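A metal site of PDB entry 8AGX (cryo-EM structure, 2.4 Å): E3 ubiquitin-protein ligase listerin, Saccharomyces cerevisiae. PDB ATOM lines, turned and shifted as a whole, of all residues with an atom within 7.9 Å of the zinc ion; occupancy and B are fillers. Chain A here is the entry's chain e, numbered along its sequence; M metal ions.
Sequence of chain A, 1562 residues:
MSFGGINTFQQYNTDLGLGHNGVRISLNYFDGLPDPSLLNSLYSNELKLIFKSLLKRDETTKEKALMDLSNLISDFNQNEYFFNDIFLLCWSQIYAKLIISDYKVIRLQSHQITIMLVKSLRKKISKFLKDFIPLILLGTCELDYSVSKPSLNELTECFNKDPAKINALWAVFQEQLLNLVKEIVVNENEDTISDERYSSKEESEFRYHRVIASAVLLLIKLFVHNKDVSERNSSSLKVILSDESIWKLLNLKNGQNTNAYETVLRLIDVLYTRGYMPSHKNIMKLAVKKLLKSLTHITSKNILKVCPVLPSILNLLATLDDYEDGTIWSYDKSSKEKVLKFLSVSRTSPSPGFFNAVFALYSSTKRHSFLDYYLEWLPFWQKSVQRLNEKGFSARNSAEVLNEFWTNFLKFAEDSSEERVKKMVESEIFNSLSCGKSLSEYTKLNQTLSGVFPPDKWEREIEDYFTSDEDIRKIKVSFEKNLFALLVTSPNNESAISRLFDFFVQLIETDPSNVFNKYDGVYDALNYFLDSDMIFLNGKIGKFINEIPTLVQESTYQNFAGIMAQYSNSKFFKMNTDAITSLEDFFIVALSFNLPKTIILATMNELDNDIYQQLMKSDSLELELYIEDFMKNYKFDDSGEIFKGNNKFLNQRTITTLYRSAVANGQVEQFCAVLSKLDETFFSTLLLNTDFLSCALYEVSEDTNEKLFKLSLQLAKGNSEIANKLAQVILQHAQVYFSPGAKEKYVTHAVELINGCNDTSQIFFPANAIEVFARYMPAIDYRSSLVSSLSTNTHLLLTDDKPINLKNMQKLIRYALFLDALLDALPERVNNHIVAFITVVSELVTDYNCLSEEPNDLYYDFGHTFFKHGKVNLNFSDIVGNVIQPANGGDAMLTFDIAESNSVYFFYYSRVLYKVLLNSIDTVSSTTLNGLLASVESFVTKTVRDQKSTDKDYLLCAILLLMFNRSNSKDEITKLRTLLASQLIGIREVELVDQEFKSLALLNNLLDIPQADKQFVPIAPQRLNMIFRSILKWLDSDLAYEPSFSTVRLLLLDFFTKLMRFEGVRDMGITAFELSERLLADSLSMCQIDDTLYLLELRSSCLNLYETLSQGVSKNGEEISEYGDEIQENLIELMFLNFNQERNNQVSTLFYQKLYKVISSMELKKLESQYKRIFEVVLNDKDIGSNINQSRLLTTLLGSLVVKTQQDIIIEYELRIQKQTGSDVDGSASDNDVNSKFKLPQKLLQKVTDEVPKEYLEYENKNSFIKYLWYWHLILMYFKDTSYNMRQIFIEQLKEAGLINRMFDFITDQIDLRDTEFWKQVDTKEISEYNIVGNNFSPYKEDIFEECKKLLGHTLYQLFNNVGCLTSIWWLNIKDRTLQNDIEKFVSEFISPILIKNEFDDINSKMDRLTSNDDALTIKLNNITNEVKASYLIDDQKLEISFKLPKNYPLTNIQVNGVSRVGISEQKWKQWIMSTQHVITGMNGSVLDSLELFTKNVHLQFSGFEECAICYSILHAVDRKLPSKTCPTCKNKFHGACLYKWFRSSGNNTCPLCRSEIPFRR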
ATOM      1  N   GLU A1506     -14.023   7.103 -22.874  1.00  0.00           N
ATOM      2  CA  GLU A1506     -13.636   8.060 -21.862  1.00  0.00           C
ATOM      3  C   GLU A1506     -13.088   9.326 -22.469  1.00  0.00           C
ATOM      4  O   GLU A1506     -12.290   9.257 -23.387  1.00  0.00           O
ATOM      5  CB  GLU A1506     -12.566   7.456 -20.966  1.00  0.00           C
ATOM      6  CG  GLU A1506     -12.748   5.984 -20.676  1.00  0.00           C
ATOM      7  CD  GLU A1506     -11.582   5.407 -19.882  1.00  0.00           C
ATOM      8  OE1 GLU A1506     -10.771   6.200 -19.367  1.00  0.00           O
ATOM      9  OE2 GLU A1506     -11.485   4.169 -19.785  1.00  0.00           O
ATOM     10  N   GLU A1507     -13.491  10.486 -21.956  1.00  0.00           N
ATOM     11  CA  GLU A1507     -12.922  11.737 -22.426  1.00  0.00           C
ATOM     12  C   GLU A1507     -11.504  11.815 -21.893  1.00  0.00           C
ATOM     13  O   GLU A1507     -11.196  11.272 -20.840  1.00  0.00           O
ATOM     14  CB  GLU A1507     -13.736  12.896 -21.896  1.00  0.00           C
ATOM     15  CG  GLU A1507     -15.228  12.688 -22.031  1.00  0.00           C
ATOM     16  CD  GLU A1507     -16.021  13.930 -21.704  1.00  0.00           C
ATOM     17  OE1 GLU A1507     -15.410  14.897 -21.201  1.00  0.00           O
ATOM     18  OE2 GLU A1507     -17.247  13.942 -21.947  1.00  0.00           O
ATOM     19  N   CYS A1508     -10.623  12.496 -22.605  1.00  0.00           N
ATOM     20  CA  CYS A1508      -9.262  12.593 -22.160  1.00  0.00           C
ATOM     21  C   CYS A1508      -9.001  13.480 -20.977  1.00  0.00           C
ATOM     22  O   CYS A1508      -9.610  14.515 -20.846  1.00  0.00           O
ATOM     23  CB  CYS A1508      -8.386  12.946 -23.318  1.00  0.00           C
ATOM     24  SG  CYS A1508      -6.906  13.838 -22.949  1.00  0.00           S
ATOM     25  N   ALA A1509      -8.091  13.069 -20.097  1.00  0.00           N
ATOM     26  CA  ALA A1509      -7.849  13.814 -18.873  1.00  0.00           C
ATOM     27  C   ALA A1509      -7.282  15.214 -19.025  1.00  0.00           C
ATOM     28  O   ALA A1509      -7.728  16.141 -18.355  1.00  0.00           O
ATOM     29  CB  ALA A1509      -6.934  13.004 -17.995  1.00  0.00           C
ATOM     30  N   ILE A1510      -6.305  15.388 -19.882  1.00  0.00           N
ATOM     31  CA  ILE A1510      -5.733  16.690 -20.098  1.00  0.00           C
ATOM     32  C   ILE A1510      -6.722  17.654 -20.705  1.00  0.00           C
ATOM     33  O   ILE A1510      -6.861  18.768 -20.231  1.00  0.00           O
ATOM     34  CB  ILE A1510      -4.496  16.599 -20.980  1.00  0.00           C
ATOM     35  CG1 ILE A1510      -3.461  15.690 -20.311  1.00  0.00           C
ATOM     36  CG2 ILE A1510      -3.903  17.963 -21.261  1.00  0.00           C
ATOM     37  CD1 ILE A1510      -2.052  15.888 -20.804  1.00  0.00           C
ATOM     38  N   CYS A1511      -7.471  17.229 -21.711  1.00  0.00           N
ATOM     39  CA  CYS A1511      -8.343  18.144 -22.410  1.00  0.00           C
ATOM     40  C   CYS A1511      -9.838  18.039 -22.244  1.00  0.00           C
ATOM     41  O   CYS A1511     -10.563  18.812 -22.839  1.00  0.00           O
ATOM     42  CB  CYS A1511      -8.051  18.063 -23.889  1.00  0.00           C
ATOM     43  SG  CYS A1511      -8.863  16.700 -24.715  1.00  0.00           S
ATOM     44  N   TYR A1512     -10.301  17.070 -21.485  1.00  0.00           N
ATOM     45  CA  TYR A1512     -11.726  16.930 -21.222  1.00  0.00           C
ATOM     46  C   TYR A1512     -12.631  16.889 -22.459  1.00  0.00           C
ATOM     47  O   TYR A1512     -13.671  17.512 -22.472  1.00  0.00           O
ATOM     48  CB  TYR A1512     -12.185  17.977 -20.213  1.00  0.00           C
ATOM     49  CG  TYR A1512     -11.317  18.021 -18.973  1.00  0.00           C
ATOM     50  CD1 TYR A1512     -11.308  16.980 -18.065  1.00  0.00           C
ATOM     51  CD2 TYR A1512     -10.485  19.110 -18.735  1.00  0.00           C
ATOM     52  CE1 TYR A1512     -10.512  17.023 -16.941  1.00  0.00           C
ATOM     53  CE2 TYR A1512      -9.689  19.153 -17.610  1.00  0.00           C
ATOM     54  CZ  TYR A1512      -9.708  18.113 -16.716  1.00  0.00           C
ATOM     55  OH  TYR A1512      -8.907  18.154 -15.601  1.00  0.00           O
ATOM     56  N   SER A1513     -12.221  16.163 -23.489  1.00  0.00           N
ATOM     57  CA  SER A1513     -13.032  16.002 -24.696  1.00  0.00           C
ATOM     58  C   SER A1513     -12.747  14.637 -25.256  1.00  0.00           C
ATOM     59  O   SER A1513     -11.726  14.061 -24.942  1.00  0.00           O
ATOM     60  CB  SER A1513     -12.673  17.055 -25.712  1.00  0.00           C
ATOM     61  OG  SER A1513     -11.414  16.780 -26.288  1.00  0.00           O
ATOM     62  N   ILE A1514     -13.648  14.093 -26.052  1.00  0.00           N
ATOM     63  CA  ILE A1514     -13.460  12.722 -26.547  1.00  0.00           C
ATOM     64  C   ILE A1514     -12.770  12.666 -27.883  1.00  0.00           C
ATOM     65  O   ILE A1514     -12.266  11.629 -28.282  1.00  0.00           O
ATOM     66  CB  ILE A1514     -14.777  11.967 -26.624  1.00  0.00           C
ATOM     67  CG1 ILE A1514     -15.785  12.569 -25.657  1.00  0.00           C
ATOM     68  CG2 ILE A1514     -14.570  10.501 -26.306  1.00  0.00           C
ATOM     69  CD1 ILE A1514     -17.006  11.709 -25.423  1.00  0.00           C
ATOM     70  N   LEU A1515     -12.757  13.780 -28.597  1.00  0.00           N
ATOM     71  CA  LEU A1515     -12.052  13.819 -29.858  1.00  0.00           C
ATOM     72  C   LEU A1515     -11.082  14.979 -29.841  1.00  0.00           C
ATOM     73  O   LEU A1515     -11.439  16.072 -29.430  1.00  0.00           O
ATOM     74  CB  LEU A1515     -13.032  13.927 -31.017  1.00  0.00           C
ATOM     75  CG  LEU A1515     -13.909  12.732 -31.355  1.00  0.00           C
ATOM     76  CD1 LEU A1515     -14.963  13.110 -32.372  1.00  0.00           C
ATOM     77  CD2 LEU A1515     -13.073  11.581 -31.864  1.00  0.00           C
ATOM     78  N   HIS A1516      -9.841  14.747 -30.262  1.00  0.00           N
ATOM     79  CA  HIS A1516      -8.849  15.802 -30.220  1.00  0.00           C
ATOM     80  C   HIS A1516      -9.318  16.851 -31.161  1.00  0.00           C
ATOM     81  O   HIS A1516      -9.796  16.542 -32.235  1.00  0.00           O
ATOM     82  CB  HIS A1516      -7.505  15.269 -30.674  1.00  0.00           C
ATOM     83  CG  HIS A1516      -6.363  16.199 -30.370  1.00  0.00           C
ATOM     84  ND1 HIS A1516      -5.882  17.101 -31.292  1.00  0.00           N
ATOM     85  CD2 HIS A1516      -5.618  16.353 -29.263  1.00  0.00           C
ATOM     86  CE1 HIS A1516      -4.880  17.773 -30.755  1.00  0.00           C
ATOM     87  NE2 HIS A1516      -4.704  17.340 -29.523  1.00  0.00           N
ATOM     88  N   ALA A1517      -9.207  18.112 -30.782  1.00  0.00           N
ATOM     89  CA  ALA A1517      -9.761  19.145 -31.628  1.00  0.00           C
ATOM     90  C   ALA A1517      -9.092  19.207 -32.978  1.00  0.00           C
ATOM     91  O   ALA A1517      -9.763  19.259 -33.994  1.00  0.00           O
ATOM     92  CB  ALA A1517      -9.625  20.485 -30.941  1.00  0.00           C
ATOM     93  N   LYS A1521      -9.298  12.502 -33.096  1.00  0.00           N
ATOM     94  CA  LYS A1521      -9.016  11.117 -32.773  1.00  0.00           C
ATOM     95  C   LYS A1521      -9.451  10.769 -31.379  1.00  0.00           C
ATOM     96  O   LYS A1521      -9.575  11.628 -30.536  1.00  0.00           O
ATOM     97  CB  LYS A1521      -7.535  10.833 -32.884  1.00  0.00           C
ATOM     98  CG  LYS A1521      -6.997  10.707 -34.288  1.00  0.00           C
ATOM     99  CD  LYS A1521      -5.519  10.377 -34.237  1.00  0.00           C
ATOM    100  CE  LYS A1521      -4.946  10.107 -35.616  1.00  0.00           C
ATOM    101  NZ  LYS A1521      -3.568   9.566 -35.521  1.00  0.00           N
ATOM    102  N   LEU A1522      -9.695   9.500 -31.147  1.00  0.00           N
ATOM    103  CA  LEU A1522     -10.140   9.034 -29.844  1.00  0.00           C
ATOM    104  C   LEU A1522      -8.983   8.989 -28.886  1.00  0.00           C
ATOM    105  O   LEU A1522      -7.834   9.023 -29.298  1.00  0.00           O
ATOM    106  CB  LEU A1522     -10.805   7.666 -29.995  1.00  0.00           C
ATOM    107  CG  LEU A1522     -12.246   7.653 -30.503  1.00  0.00           C
ATOM    108  CD1 LEU A1522     -12.706   6.218 -30.677  1.00  0.00           C
ATOM    109  CD2 LEU A1522     -13.150   8.393 -29.535  1.00  0.00           C
ATOM    110  N   PRO A1523      -9.259   8.893 -27.590  1.00  0.00           N
ATOM    111  CA  PRO A1523      -8.118   8.955 -26.699  1.00  0.00           C
ATOM    112  C   PRO A1523      -7.389   7.650 -26.576  1.00  0.00           C
ATOM    113  O   PRO A1523      -7.715   6.851 -25.712  1.00  0.00           O
ATOM    114  CB  PRO A1523      -8.755   9.306 -25.363  1.00  0.00           C
ATOM    115  CG  PRO A1523     -10.011  10.012 -25.712  1.00  0.00           C
ATOM    116  CD  PRO A1523     -10.510   9.262 -26.898  1.00  0.00           C
ATOM    117  N   LYS A1533      -7.233   7.812 -19.566  1.00  0.00           N
ATOM    118  CA  LYS A1533      -7.062   7.793 -21.025  1.00  0.00           C
ATOM    119  C   LYS A1533      -6.743   9.129 -21.611  1.00  0.00           C
ATOM    120  O   LYS A1533      -7.447  10.091 -21.350  1.00  0.00           O
ATOM    121  CB  LYS A1533      -8.303   7.236 -21.699  1.00  0.00           C
ATOM    122  CG  LYS A1533      -8.253   5.736 -21.909  1.00  0.00           C
ATOM    123  CD  LYS A1533      -9.357   5.272 -22.842  1.00  0.00           C
ATOM    124  CE  LYS A1533      -9.267   3.772 -23.088  1.00  0.00           C
ATOM    125  NZ  LYS A1533     -10.375   3.275 -23.940  1.00  0.00           N
ATOM    126  N   PHE A1534      -5.708   9.205 -22.449  1.00  0.00           N
ATOM    127  CA  PHE A1534      -5.260  10.479 -22.973  1.00  0.00           C
ATOM    128  C   PHE A1534      -5.103  10.481 -24.465  1.00  0.00           C
ATOM    129  O   PHE A1534      -4.794   9.452 -25.043  1.00  0.00           O
ATOM    130  CB  PHE A1534      -3.885  10.836 -22.419  1.00  0.00           C
ATOM    131  CG  PHE A1534      -3.748  10.696 -20.940  1.00  0.00           C
ATOM    132  CD1 PHE A1534      -4.090  11.728 -20.096  1.00  0.00           C
ATOM    133  CD2 PHE A1534      -3.239   9.528 -20.394  1.00  0.00           C
ATOM    134  CE1 PHE A1534      -3.951  11.602 -18.731  1.00  0.00           C
ATOM    135  CE2 PHE A1534      -3.098   9.394 -19.027  1.00  0.00           C
ATOM    136  CZ  PHE A1534      -3.449  10.441 -18.200  1.00  0.00           C
ATOM    137  N   HIS A1535      -5.340  11.621 -25.106  1.00  0.00           N
ATOM    138  CA  HIS A1535      -5.077  11.716 -26.521  1.00  0.00           C
ATOM    139  C   HIS A1535      -3.596  11.731 -26.570  1.00  0.00           C
ATOM    140  O   HIS A1535      -2.955  12.280 -25.692  1.00  0.00           O
ATOM    141  CB  HIS A1535      -5.620  12.999 -27.123  1.00  0.00           C
ATOM    142  CG  HIS A1535      -7.102  13.049 -27.242  1.00  0.00           C
ATOM    143  ND1 HIS A1535      -7.872  13.974 -26.591  1.00  0.00           N
ATOM    144  CD2 HIS A1535      -7.953  12.282 -27.962  1.00  0.00           C
ATOM    145  CE1 HIS A1535      -9.149  13.780 -26.902  1.00  0.00           C
ATOM    146  NE2 HIS A1535      -9.219  12.757 -27.731  1.00  0.00           N
ATOM    147  N   GLY A1536      -3.026  11.154 -27.605  1.00  0.00           N
ATOM    148  CA  GLY A1536      -1.579  11.048 -27.644  1.00  0.00           C
ATOM    149  C   GLY A1536      -0.973  12.421 -27.637  1.00  0.00           C
ATOM    150  O   GLY A1536      -0.098  12.686 -26.840  1.00  0.00           O
ATOM    151  N   ALA A1537      -1.512  13.323 -28.424  1.00  0.00           N
ATOM    152  CA  ALA A1537      -0.984  14.660 -28.498  1.00  0.00           C
ATOM    153  C   ALA A1537      -1.064  15.425 -27.168  1.00  0.00           C
ATOM    154  O   ALA A1537      -0.098  16.073 -26.781  1.00  0.00           O
ATOM    155  CB  ALA A1537      -1.707  15.412 -29.574  1.00  0.00           C
ATOM    156  N   CYS A1538      -2.180  15.322 -26.458  1.00  0.00           N
ATOM    157  CA  CYS A1538      -2.304  16.008 -25.198  1.00  0.00           C
ATOM    158  C   CYS A1538      -1.186  15.486 -24.266  1.00  0.00           C
ATOM    159  O   CYS A1538      -0.483  16.285 -23.671  1.00  0.00           O
ATOM    160  CB  CYS A1538      -3.699  15.765 -24.557  1.00  0.00           C
ATOM    161  SG  CYS A1538      -5.267  16.080 -25.466  1.00  0.00           S
ATOM    162  N   LEU A1539      -0.989  14.181 -24.188  1.00  0.00           N
ATOM    163  CA  LEU A1539       0.031  13.596 -23.298  1.00  0.00           C
ATOM    164  C   LEU A1539       1.416  13.929 -23.685  1.00  0.00           C
ATOM    165  O   LEU A1539       2.251  14.200 -22.830  1.00  0.00           O
ATOM    166  CB  LEU A1539      -0.058  12.082 -23.350  1.00  0.00           C
ATOM    167  CG  LEU A1539       0.694  11.250 -22.327  1.00  0.00           C
ATOM    168  CD1 LEU A1539       0.175  11.528 -20.922  1.00  0.00           C
ATOM    169  CD2 LEU A1539       0.558   9.768 -22.645  1.00  0.00           C
HETATM  170 ZN    ZN M   1      -7.323  14.981 -24.904  1.00  0.00          ZN
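A ring nitrogen (NE2) of His 1535 is in hydrogen-bond range of the backbone carbonyl oxygen (O) of Ile 1514.
The side-chain sulfur (SG) of Cys 1508 sits close to the backbone NH (N) of Ile 1510.
The backbone carbonyl oxygen (O) of Ser 1513 lies within hydrogen-bond range of the backbone NH (N) of Cys 1508, at 3.0 Å.
N of His 1516 is in hydrogen-bond range of NE2 of His 1535 (3.3 Å).
The side-chain hydroxyl (OG) of Ser 1513 lies close to the side-chain sulfur (SG) of Cys 1511.
The backbone carbonyl oxygen (O) of Lys 1521 sits at hydrogen-bond distance from a ring nitrogen (NE2) of His 1535 (3.0 Å).
The zinc ion is bound by a ring nitrogen (ND1) of His 1535 (2.0 Å).
The side-chain sulfur (SG) of Cys 1508 binds the zinc ion, at 2.3 Å.
SG of Cys 1511 binds the zinc ion, 2.3 Å away.
The zinc ion is bound by SG of Cys 1538 (2.4 Å).
The zinc ion has four donor atoms within binding distance.
The nearest printed residue that does not touch the zinc ion is Ser 1513 (4.5 Å).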
